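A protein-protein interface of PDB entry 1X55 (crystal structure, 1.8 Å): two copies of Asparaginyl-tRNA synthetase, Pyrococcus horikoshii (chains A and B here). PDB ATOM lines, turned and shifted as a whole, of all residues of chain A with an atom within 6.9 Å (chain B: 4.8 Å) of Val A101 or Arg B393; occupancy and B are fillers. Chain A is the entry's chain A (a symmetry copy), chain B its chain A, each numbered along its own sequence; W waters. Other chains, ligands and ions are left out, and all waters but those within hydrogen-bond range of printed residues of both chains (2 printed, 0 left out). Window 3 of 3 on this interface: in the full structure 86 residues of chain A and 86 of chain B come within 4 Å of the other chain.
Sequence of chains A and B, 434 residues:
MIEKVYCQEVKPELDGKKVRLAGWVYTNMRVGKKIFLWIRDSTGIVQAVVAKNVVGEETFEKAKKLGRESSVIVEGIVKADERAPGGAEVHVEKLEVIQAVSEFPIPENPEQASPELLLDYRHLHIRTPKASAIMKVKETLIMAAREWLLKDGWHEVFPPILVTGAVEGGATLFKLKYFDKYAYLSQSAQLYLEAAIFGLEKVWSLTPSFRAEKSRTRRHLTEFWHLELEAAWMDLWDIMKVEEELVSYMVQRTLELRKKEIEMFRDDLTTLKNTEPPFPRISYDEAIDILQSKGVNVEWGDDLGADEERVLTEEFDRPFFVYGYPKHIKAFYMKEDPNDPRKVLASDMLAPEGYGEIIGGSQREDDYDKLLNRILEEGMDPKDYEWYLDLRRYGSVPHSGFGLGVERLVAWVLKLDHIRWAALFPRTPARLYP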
ATOM      1  N   TRP A  24      16.145  11.922 -23.354  1.00  0.00           N
ATOM      2  CA  TRP A  24      17.327  11.709 -22.538  1.00  0.00           C
ATOM      3  C   TRP A  24      16.923  11.211 -21.153  1.00  0.00           C
ATOM      4  O   TRP A  24      15.910  11.662 -20.597  1.00  0.00           O
ATOM      5  CB  TRP A  24      18.134  13.016 -22.430  1.00  0.00           C
ATOM      6  CG  TRP A  24      18.664  13.468 -23.782  1.00  0.00           C
ATOM      7  CD1 TRP A  24      19.867  13.162 -24.342  1.00  0.00           C
ATOM      8  CD2 TRP A  24      17.992  14.310 -24.714  1.00  0.00           C
ATOM      9  NE1 TRP A  24      19.986  13.752 -25.580  1.00  0.00           N
ATOM     10  CE2 TRP A  24      18.834  14.452 -25.841  1.00  0.00           C
ATOM     11  CE3 TRP A  24      16.726  14.931 -24.734  1.00  0.00           C
ATOM     12  CZ2 TRP A  24      18.474  15.215 -26.963  1.00  0.00           C
ATOM     13  CZ3 TRP A  24      16.349  15.683 -25.875  1.00  0.00           C
ATOM     14  CH2 TRP A  24      17.220  15.818 -26.966  1.00  0.00           C
ATOM     15  N   LYS A  65      22.183   0.109 -17.112  1.00  0.00           N
ATOM     16  CA  LYS A  65      23.401   0.876 -17.195  1.00  0.00           C
ATOM     17  C   LYS A  65      23.187   2.320 -17.652  1.00  0.00           C
ATOM     18  O   LYS A  65      24.149   3.060 -17.776  1.00  0.00           O
ATOM     19  CB  LYS A  65      24.395   0.155 -18.105  1.00  0.00           C
ATOM     20  CG  LYS A  65      24.898  -1.150 -17.498  1.00  0.00           C
ATOM     21  CD  LYS A  65      26.069  -1.706 -18.304  1.00  0.00           C
ATOM     22  CE  LYS A  65      25.593  -2.463 -19.551  1.00  0.00           C
ATOM     23  NZ  LYS A  65      25.425  -3.948 -19.298  1.00  0.00           N
ATOM     24  N   LEU A  66      21.940   2.723 -17.908  1.00  0.00           N
ATOM     25  CA  LEU A  66      21.689   4.040 -18.496  1.00  0.00           C
ATOM     26  C   LEU A  66      21.712   5.089 -17.405  1.00  0.00           C
ATOM     27  O   LEU A  66      20.844   5.108 -16.540  1.00  0.00           O
ATOM     28  CB  LEU A  66      20.352   4.092 -19.259  1.00  0.00           C
ATOM     29  CG  LEU A  66      20.192   3.136 -20.442  1.00  0.00           C
ATOM     30  CD1 LEU A  66      18.829   3.292 -21.067  1.00  0.00           C
ATOM     31  CD2 LEU A  66      21.301   3.363 -21.485  1.00  0.00           C
ATOM     32  N   GLY A  67      22.731   5.936 -17.437  1.00  0.00           N
ATOM     33  CA  GLY A  67      22.825   7.058 -16.507  1.00  0.00           C
ATOM     34  C   GLY A  67      22.144   8.297 -17.066  1.00  0.00           C
ATOM     35  O   GLY A  67      21.612   8.290 -18.191  1.00  0.00           O
ATOM     36  N   ARG A  68      22.178   9.365 -16.274  1.00  0.00           N
ATOM     37  CA  ARG A  68      21.591  10.639 -16.652  1.00  0.00           C
ATOM     38  C   ARG A  68      22.205  11.127 -17.965  1.00  0.00           C
ATOM     39  O   ARG A  68      23.420  11.046 -18.172  1.00  0.00           O
ATOM     40  CB  ARG A  68      21.829  11.673 -15.548  1.00  0.00           C
ATOM     41  CG  ARG A  68      21.114  11.369 -14.227  1.00  0.00           C
ATOM     42  CD  ARG A  68      21.360  12.412 -13.135  1.00  0.00           C
ATOM     43  NE  ARG A  68      22.756  12.849 -13.140  1.00  0.00           N
ATOM     44  CZ  ARG A  68      23.146  14.083 -13.445  1.00  0.00           C
ATOM     45  NH1 ARG A  68      22.249  15.018 -13.736  1.00  0.00           N
ATOM     46  NH2 ARG A  68      24.437  14.382 -13.442  1.00  0.00           N
ATOM     47  N   GLU A  69      21.324  11.630 -18.824  1.00  0.00           N
ATOM     48  CA  GLU A  69      21.610  12.144 -20.177  1.00  0.00           C
ATOM     49  C   GLU A  69      21.876  11.100 -21.268  1.00  0.00           C
ATOM     50  O   GLU A  69      22.153  11.475 -22.420  1.00  0.00           O
ATOM     51  CB  GLU A  69      22.653  13.285 -20.176  1.00  0.00           C
ATOM     52  CG  GLU A  69      22.195  14.502 -19.378  1.00  0.00           C
ATOM     53  CD  GLU A  69      20.938  15.125 -19.939  1.00  0.00           C
ATOM     54  OE1 GLU A  69      20.869  15.329 -21.175  1.00  0.00           O
ATOM     55  OE2 GLU A  69      20.012  15.402 -19.153  1.00  0.00           O
ATOM     56  N   SER A  70      21.735   9.812 -20.936  1.00  0.00           N
ATOM     57  CA  SER A  70      21.713   8.765 -21.971  1.00  0.00           C
ATOM     58  C   SER A  70      20.640   9.094 -23.003  1.00  0.00           C
ATOM     59  O   SER A  70      19.486   9.354 -22.634  1.00  0.00           O
ATOM     60  CB  SER A  70      21.422   7.377 -21.364  1.00  0.00           C
ATOM     61  OG  SER A  70      22.437   6.994 -20.436  1.00  0.00           O
ATOM     62  N   SER A  71      21.010   9.084 -24.284  1.00  0.00           N
ATOM     63  CA  SER A  71      20.038   9.375 -25.328  1.00  0.00           C
ATOM     64  C   SER A  71      19.364   8.075 -25.767  1.00  0.00           C
ATOM     65  O   SER A  71      20.034   7.064 -26.053  1.00  0.00           O
ATOM     66  CB  SER A  71      20.670  10.114 -26.491  1.00  0.00           C
ATOM     67  OG  SER A  71      21.842   9.460 -26.937  1.00  0.00           O
ATOM     68  N   VAL A  97      19.059   2.322 -27.397  1.00  0.00           N
ATOM     69  CA  VAL A  97      20.024   3.180 -26.743  1.00  0.00           C
ATOM     70  C   VAL A  97      20.843   3.848 -27.834  1.00  0.00           C
ATOM     71  O   VAL A  97      21.580   3.176 -28.564  1.00  0.00           O
ATOM     72  CB  VAL A  97      20.915   2.377 -25.766  1.00  0.00           C
ATOM     73  CG1 VAL A  97      21.939   3.289 -25.075  1.00  0.00           C
ATOM     74  CG2 VAL A  97      20.027   1.652 -24.727  1.00  0.00           C
ATOM     75  N   GLN A  99      23.016   6.727 -27.202  1.00  0.00           N
ATOM     76  CA  GLN A  99      24.280   6.785 -26.507  1.00  0.00           C
ATOM     77  C   GLN A  99      24.090   6.671 -25.003  1.00  0.00           C
ATOM     78  O   GLN A  99      23.394   7.490 -24.397  1.00  0.00           O
ATOM     79  CB  GLN A  99      25.021   8.077 -26.834  1.00  0.00           C
ATOM     80  CG  GLN A  99      26.337   8.224 -26.110  1.00  0.00           C
ATOM     81  CD  GLN A  99      27.099   9.431 -26.582  1.00  0.00           C
ATOM     82  OE1 GLN A  99      26.604  10.571 -26.478  1.00  0.00           O
ATOM     83  NE2 GLN A  99      28.313   9.201 -27.108  1.00  0.00           N
ATOM     84  N   ALA A 100      24.752   5.697 -24.397  1.00  0.00           N
ATOM     85  CA  ALA A 100      24.710   5.563 -22.937  1.00  0.00           C
ATOM     86  C   ALA A 100      25.683   6.576 -22.297  1.00  0.00           C
ATOM     87  O   ALA A 100      26.752   6.841 -22.835  1.00  0.00           O
ATOM     88  CB  ALA A 100      25.061   4.130 -22.530  1.00  0.00           C
ATOM     89  N   VAL A 101      25.294   7.145 -21.168  1.00  0.00           N
ATOM     90  CA  VAL A 101      26.108   8.142 -20.474  1.00  0.00           C
ATOM     91  C   VAL A 101      26.100   7.767 -18.995  1.00  0.00           C
ATOM     92  O   VAL A 101      25.065   7.386 -18.456  1.00  0.00           O
ATOM     93  CB  VAL A 101      25.522   9.573 -20.663  1.00  0.00           C
ATOM     94  CG1 VAL A 101      26.338  10.609 -19.925  1.00  0.00           C
ATOM     95  CG2 VAL A 101      25.439   9.938 -22.152  1.00  0.00           C
ATOM     96  N   SER A 102      27.229   7.925 -18.322  1.00  0.00           N
ATOM     97  CA  SER A 102      27.259   7.640 -16.891  1.00  0.00           C
ATOM     98  C   SER A 102      27.903   8.762 -16.073  1.00  0.00           C
ATOM     99  O   SER A 102      27.796   8.773 -14.842  1.00  0.00           O
ATOM    100  CB  SER A 102      27.929   6.288 -16.629  1.00  0.00           C
ATOM    101  OG  SER A 102      29.252   6.278 -17.120  1.00  0.00           O
ATOM    102  N   GLU A 103      28.540   9.713 -16.752  1.00  0.00           N
ATOM    103  CA  GLU A 103      29.275  10.776 -16.067  1.00  0.00           C
ATOM    104  C   GLU A 103      28.950  12.200 -16.537  1.00  0.00           C
ATOM    105  O   GLU A 103      29.844  13.004 -16.780  1.00  0.00           O
ATOM    106  CB  GLU A 103      30.777  10.529 -16.186  1.00  0.00           C
ATOM    107  CG  GLU A 103      31.197   9.145 -15.723  1.00  0.00           C
ATOM    108  CD  GLU A 103      32.672   8.925 -15.906  1.00  0.00           C
ATOM    109  OE1 GLU A 103      33.385   8.906 -14.881  1.00  0.00           O
ATOM    110  OE2 GLU A 103      33.113   8.802 -17.069  1.00  0.00           O
ATOM    111  N   PHE A 104      27.669  12.528 -16.629  1.00  0.00           N
ATOM    112  CA  PHE A 104      27.288  13.894 -16.974  1.00  0.00           C
ATOM    113  C   PHE A 104      27.838  14.833 -15.900  1.00  0.00           C
ATOM    114  O   PHE A 104      27.568  14.600 -14.729  1.00  0.00           O
ATOM    115  CB  PHE A 104      25.772  13.997 -17.052  1.00  0.00           C
ATOM    116  CG  PHE A 104      25.287  15.264 -17.679  1.00  0.00           C
ATOM    117  CD1 PHE A 104      25.674  15.601 -18.978  1.00  0.00           C
ATOM    118  CD2 PHE A 104      24.416  16.103 -16.996  1.00  0.00           C
ATOM    119  CE1 PHE A 104      25.209  16.754 -19.581  1.00  0.00           C
ATOM    120  CE2 PHE A 104      23.944  17.272 -17.603  1.00  0.00           C
ATOM    121  CZ  PHE A 104      24.341  17.584 -18.902  1.00  0.00           C
ATOM    122  N   PRO A 105      28.644  15.833 -16.270  1.00  0.00           N
ATOM    123  CA  PRO A 105      29.323  16.683 -15.274  1.00  0.00           C
ATOM    124  C   PRO A 105      28.494  17.763 -14.585  1.00  0.00           C
ATOM    125  O   PRO A 105      29.025  18.466 -13.743  1.00  0.00           O
ATOM    126  CB  PRO A 105      30.448  17.348 -16.071  1.00  0.00           C
ATOM    127  CG  PRO A 105      29.999  17.335 -17.486  1.00  0.00           C
ATOM    128  CD  PRO A 105      29.027  16.195 -17.649  1.00  0.00           C
ATOM    129  N   ARG A 127      20.796  22.695 -20.931  1.00  0.00           N
ATOM    130  CA  ARG A 127      19.764  21.681 -21.203  1.00  0.00           C
ATOM    131  C   ARG A 127      18.967  21.303 -19.949  1.00  0.00           C
ATOM    132  O   ARG A 127      17.943  20.614 -20.063  1.00  0.00           O
ATOM    133  CB  ARG A 127      20.343  20.420 -21.852  1.00  0.00           C
ATOM    134  CG  ARG A 127      21.126  19.559 -20.918  1.00  0.00           C
ATOM    135  CD  ARG A 127      21.646  18.277 -21.569  1.00  0.00           C
ATOM    136  NE  ARG A 127      22.669  18.497 -22.587  1.00  0.00           N
ATOM    137  CZ  ARG A 127      23.332  17.518 -23.191  1.00  0.00           C
ATOM    138  NH1 ARG A 127      23.090  16.243 -22.856  1.00  0.00           N
ATOM    139  NH2 ARG A 127      24.263  17.806 -24.099  1.00  0.00           N
ATOM    140  N   TYR B 368      31.494  11.099 -32.144  1.00  0.00           N
ATOM    141  CA  TYR B 368      32.607  11.791 -31.507  1.00  0.00           C
ATOM    142  C   TYR B 368      33.919  11.577 -32.255  1.00  0.00           C
ATOM    143  O   TYR B 368      34.611  12.540 -32.582  1.00  0.00           O
ATOM    144  CB  TYR B 368      32.786  11.331 -30.054  1.00  0.00           C
ATOM    145  CG  TYR B 368      33.988  11.941 -29.384  1.00  0.00           C
ATOM    146  CD1 TYR B 368      35.257  11.355 -29.500  1.00  0.00           C
ATOM    147  CD2 TYR B 368      33.874  13.111 -28.642  1.00  0.00           C
ATOM    148  CE1 TYR B 368      36.365  11.925 -28.891  1.00  0.00           C
ATOM    149  CE2 TYR B 368      34.975  13.682 -28.025  1.00  0.00           C
ATOM    150  CZ  TYR B 368      36.217  13.090 -28.150  1.00  0.00           C
ATOM    151  OH  TYR B 368      37.294  13.685 -27.508  1.00  0.00           O
ATOM    152  N   LEU B 389      32.528  19.117 -29.086  1.00  0.00           N
ATOM    153  CA  LEU B 389      32.746  17.667 -29.010  1.00  0.00           C
ATOM    154  C   LEU B 389      31.952  16.997 -27.861  1.00  0.00           C
ATOM    155  O   LEU B 389      31.474  15.860 -28.021  1.00  0.00           O
ATOM    156  CB  LEU B 389      34.244  17.341 -28.903  1.00  0.00           C
ATOM    157  CG  LEU B 389      35.071  17.522 -30.185  1.00  0.00           C
ATOM    158  CD1 LEU B 389      36.547  17.797 -29.827  1.00  0.00           C
ATOM    159  CD2 LEU B 389      34.953  16.308 -31.098  1.00  0.00           C
ATOM    160  N   ASP B 390      31.820  17.693 -26.725  1.00  0.00           N
ATOM    161  CA  ASP B 390      31.010  17.230 -25.592  1.00  0.00           C
ATOM    162  C   ASP B 390      29.599  16.858 -26.036  1.00  0.00           C
ATOM    163  O   ASP B 390      28.976  15.956 -25.456  1.00  0.00           O
ATOM    164  CB  ASP B 390      30.871  18.312 -24.506  1.00  0.00           C
ATOM    165  CG  ASP B 390      32.087  18.410 -23.593  1.00  0.00           C
ATOM    166  OD1 ASP B 390      32.981  17.520 -23.641  1.00  0.00           O
ATOM    167  OD2 ASP B 390      32.224  19.360 -22.792  1.00  0.00           O
ATOM    168  N   LEU B 391      29.089  17.548 -27.065  1.00  0.00           N
ATOM    169  CA  LEU B 391      27.727  17.264 -27.523  1.00  0.00           C
ATOM    170  C   LEU B 391      27.609  15.869 -28.162  1.00  0.00           C
ATOM    171  O   LEU B 391      26.500  15.357 -28.368  1.00  0.00           O
ATOM    172  CB  LEU B 391      27.218  18.356 -28.472  1.00  0.00           C
ATOM    173  CG  LEU B 391      27.316  19.792 -27.928  1.00  0.00           C
ATOM    174  CD1 LEU B 391      26.923  20.724 -29.085  1.00  0.00           C
ATOM    175  CD2 LEU B 391      26.434  19.983 -26.661  1.00  0.00           C
ATOM    176  N   ARG B 392      28.765  15.276 -28.476  1.00  0.00           N
ATOM    177  CA  ARG B 392      28.848  13.913 -29.013  1.00  0.00           C
ATOM    178  C   ARG B 392      29.253  12.901 -27.942  1.00  0.00           C
ATOM    179  O   ARG B 392      29.406  11.713 -28.243  1.00  0.00           O
ATOM    180  CB  ARG B 392      29.849  13.851 -30.167  1.00  0.00           C
ATOM    181  CG  ARG B 392      29.320  14.450 -31.473  1.00  0.00           C
ATOM    182  CD  ARG B 392      29.287  15.995 -31.481  1.00  0.00           C
ATOM    183  NE  ARG B 392      28.708  16.435 -32.741  1.00  0.00           N
ATOM    184  CZ  ARG B 392      28.375  17.689 -33.032  1.00  0.00           C
ATOM    185  NH1 ARG B 392      28.577  18.676 -32.137  1.00  0.00           N
ATOM    186  NH2 ARG B 392      27.825  17.932 -34.222  1.00  0.00           N
ATOM    187  N   ARG B 393      29.364  13.361 -26.697  1.00  0.00           N
ATOM    188  CA  ARG B 393      29.754  12.492 -25.577  1.00  0.00           C
ATOM    189  C   ARG B 393      28.609  12.265 -24.582  1.00  0.00           C
ATOM    190  O   ARG B 393      28.533  11.212 -23.928  1.00  0.00           O
ATOM    191  CB  ARG B 393      30.899  13.129 -24.794  1.00  0.00           C
ATOM    192  CG  ARG B 393      32.204  13.305 -25.525  1.00  0.00           C
ATOM    193  CD  ARG B 393      33.312  13.860 -24.609  1.00  0.00           C
ATOM    194  NE  ARG B 393      33.629  12.912 -23.568  1.00  0.00           N
ATOM    195  CZ  ARG B 393      34.710  12.127 -23.553  1.00  0.00           C
ATOM    196  NH1 ARG B 393      35.648  12.197 -24.512  1.00  0.00           N
ATOM    197  NH2 ARG B 393      34.863  11.277 -22.546  1.00  0.00           N
ATOM    198  N   TYR B 394      27.765  13.279 -24.426  1.00  0.00           N
ATOM    199  CA  TYR B 394      26.752  13.272 -23.364  1.00  0.00           C
ATOM    200  C   TYR B 394      25.333  13.151 -23.906  1.00  0.00           C
ATOM    201  O   TYR B 394      24.483  14.027 -23.684  1.00  0.00           O
ATOM    202  CB  TYR B 394      26.894  14.483 -22.459  1.00  0.00           C
ATOM    203  CG  TYR B 394      28.256  14.582 -21.798  1.00  0.00           C
ATOM    204  CD1 TYR B 394      28.678  13.612 -20.873  1.00  0.00           C
ATOM    205  CD2 TYR B 394      29.119  15.624 -22.095  1.00  0.00           C
ATOM    206  CE1 TYR B 394      29.921  13.690 -20.256  1.00  0.00           C
ATOM    207  CE2 TYR B 394      30.381  15.709 -21.482  1.00  0.00           C
ATOM    208  CZ  TYR B 394      30.765  14.734 -20.562  1.00  0.00           C
ATOM    209  OH  TYR B 394      31.989  14.780 -19.934  1.00  0.00           O
ATOM    210  N   GLY B 395      25.081  12.059 -24.617  1.00  0.00           N
ATOM    211  CA  GLY B 395      23.760  11.790 -25.147  1.00  0.00           C
ATOM    212  C   GLY B 395      23.563  12.322 -26.555  1.00  0.00           C
ATOM    213  O   GLY B 395      22.531  12.940 -26.861  1.00  0.00           O
HETATM  214  O   HOH W   1      25.107  15.557 -25.885  1.00  0.00           O
HETATM  215  O   HOH W   2      32.360  13.403 -17.619  1.00  0.00           O
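The indole nitrogen (NE1) of Trp A24 is in hydrogen-bond range of the backbone carbonyl oxygen (O) of Gly B395 (3.0 Å).
The backbone carbonyl oxygen (O) of Arg B392 lies within hydrogen-bond range of the side-chain amide nitrogen (NE2) of Gln A99 (3.0 Å).
The backbone NH of Gly B395 sits at hydrogen-bond distance from the side-chain amide oxygen of Gln A99 (2.8 Å).
The guanidinium group (NH1) of Arg A127 lies within hydrogen-bond range of the backbone carbonyl oxygen (O) of Tyr B394 (2.7 Å).
The side-chain amide oxygen of Gln A99 lies close to the backbone carbonyl oxygen of Arg B393, 3.3 Å away.
The backbone carbonyl oxygen of Val A101 sits at hydrogen-bond distance from the backbone NH of Gly A67 (2.9 Å).
OE1 of Glu A69 is in salt-bridge range of NH1 of Arg A127 (2.9 Å).
The backbone carbonyl oxygen (O) of Gln A99 sits at hydrogen-bond distance from the backbone NH (N) of Ser A71.
The backbone carbonyl oxygen (O) of Phe A104 sits at hydrogen-bond distance from the guanidinium group (NH2) of Arg A68, 3.4 Å away.
OG of Ser A70 lies within hydrogen-bond range of N of Val A101 (3.0 Å).
Glu A69 touches Tyr B394.
Gly B395 touches Glu A69 (CA to O, 3.2 Å).
Ser A71 touches Gly B395.
Gln A99 touches Tyr B394.
Val A101 touches Arg B393 (CG2 to O, 3.8 Å).
Tyr B394 touches Val A101 (C to CG2, 3.7 Å).
Val A101 touches Gly B395 (CG2 to N, 3.3 Å).
Tyr B394 touches Glu A103 (CE1 to O, 3.5 Å).
Phe A104 touches Tyr B394.
Pro A105 touches Tyr B394.
Val A101 touches just these residues of chain B: Arg B393, Tyr B394 and Gly B395.
Of chain A, only Gln A99 and Val A101 come within 4 Å of Arg B393.
Of the printed residues of chain B, Gln A99 touches Arg B392 (3.0 Å), Arg B393 (3.2 Å), Tyr B394 (3.6 Å) and Gly B395 (2.8 Å).
Of the printed residues of chain B, Arg A127 touches Tyr B394 (2.7 Å).
Of the printed residues of chain A, Tyr B394 touches Glu A69, Gln A99, Val A101, Glu A103, Phe A104, Pro A105 and Arg A127.
Printed residues of chain B within 4 Å of Glu A69: Tyr B394 (3.7 Å) and Gly B395 (3.2 Å).
Of the printed residues of chain B, Pro A105 touches Tyr B394 (3.7 Å).
Tyr B368 touches none of the printed residues of chain A.
The nearest printed residue of chain B that does not touch Glu A69 is Arg B393 (6.6 Å).
Printed residues of chain A that touch a printed residue of chain B: Trp A24, Glu A69, Ser A71, Gln A99, Val A101, Glu A103, Phe A104, Pro A105 and Arg A127.
Hydrophobic or aromatic side chains of chain A within 4 Å of the printed part of chain B: Trp A24, Val A101, Phe A104 and Pro A105.
Of the 8 printed residues of chain B, 4 touch a printed residue of chain A.
Hydrophobic or aromatic side chains of chain B within 4 Å of the printed part of chain A: Tyr B394.
Among the printed residues, no Asp or Glu carboxylate lies within 4 Å of a Lys or Arg side-chain nitrogen of the other chain.
No position is printed for both chains.
Of the 15 pairs that touch across the chains among the printed residues, none has its exchanged pair printed and touching as well.
Water W2 bridges the backbone carbonyl oxygen (O) of Glu A103 (2.7 Å) and the side-chain hydroxyl (OH) of Tyr B394 (2.7 Å).
Water W1 lies within hydrogen-bond range of the backbone carbonyl oxygen (O) of Tyr B394, the backbone carbonyl oxygen (O) of Leu B391 and the guanidinium group (NH2) of Arg A127.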
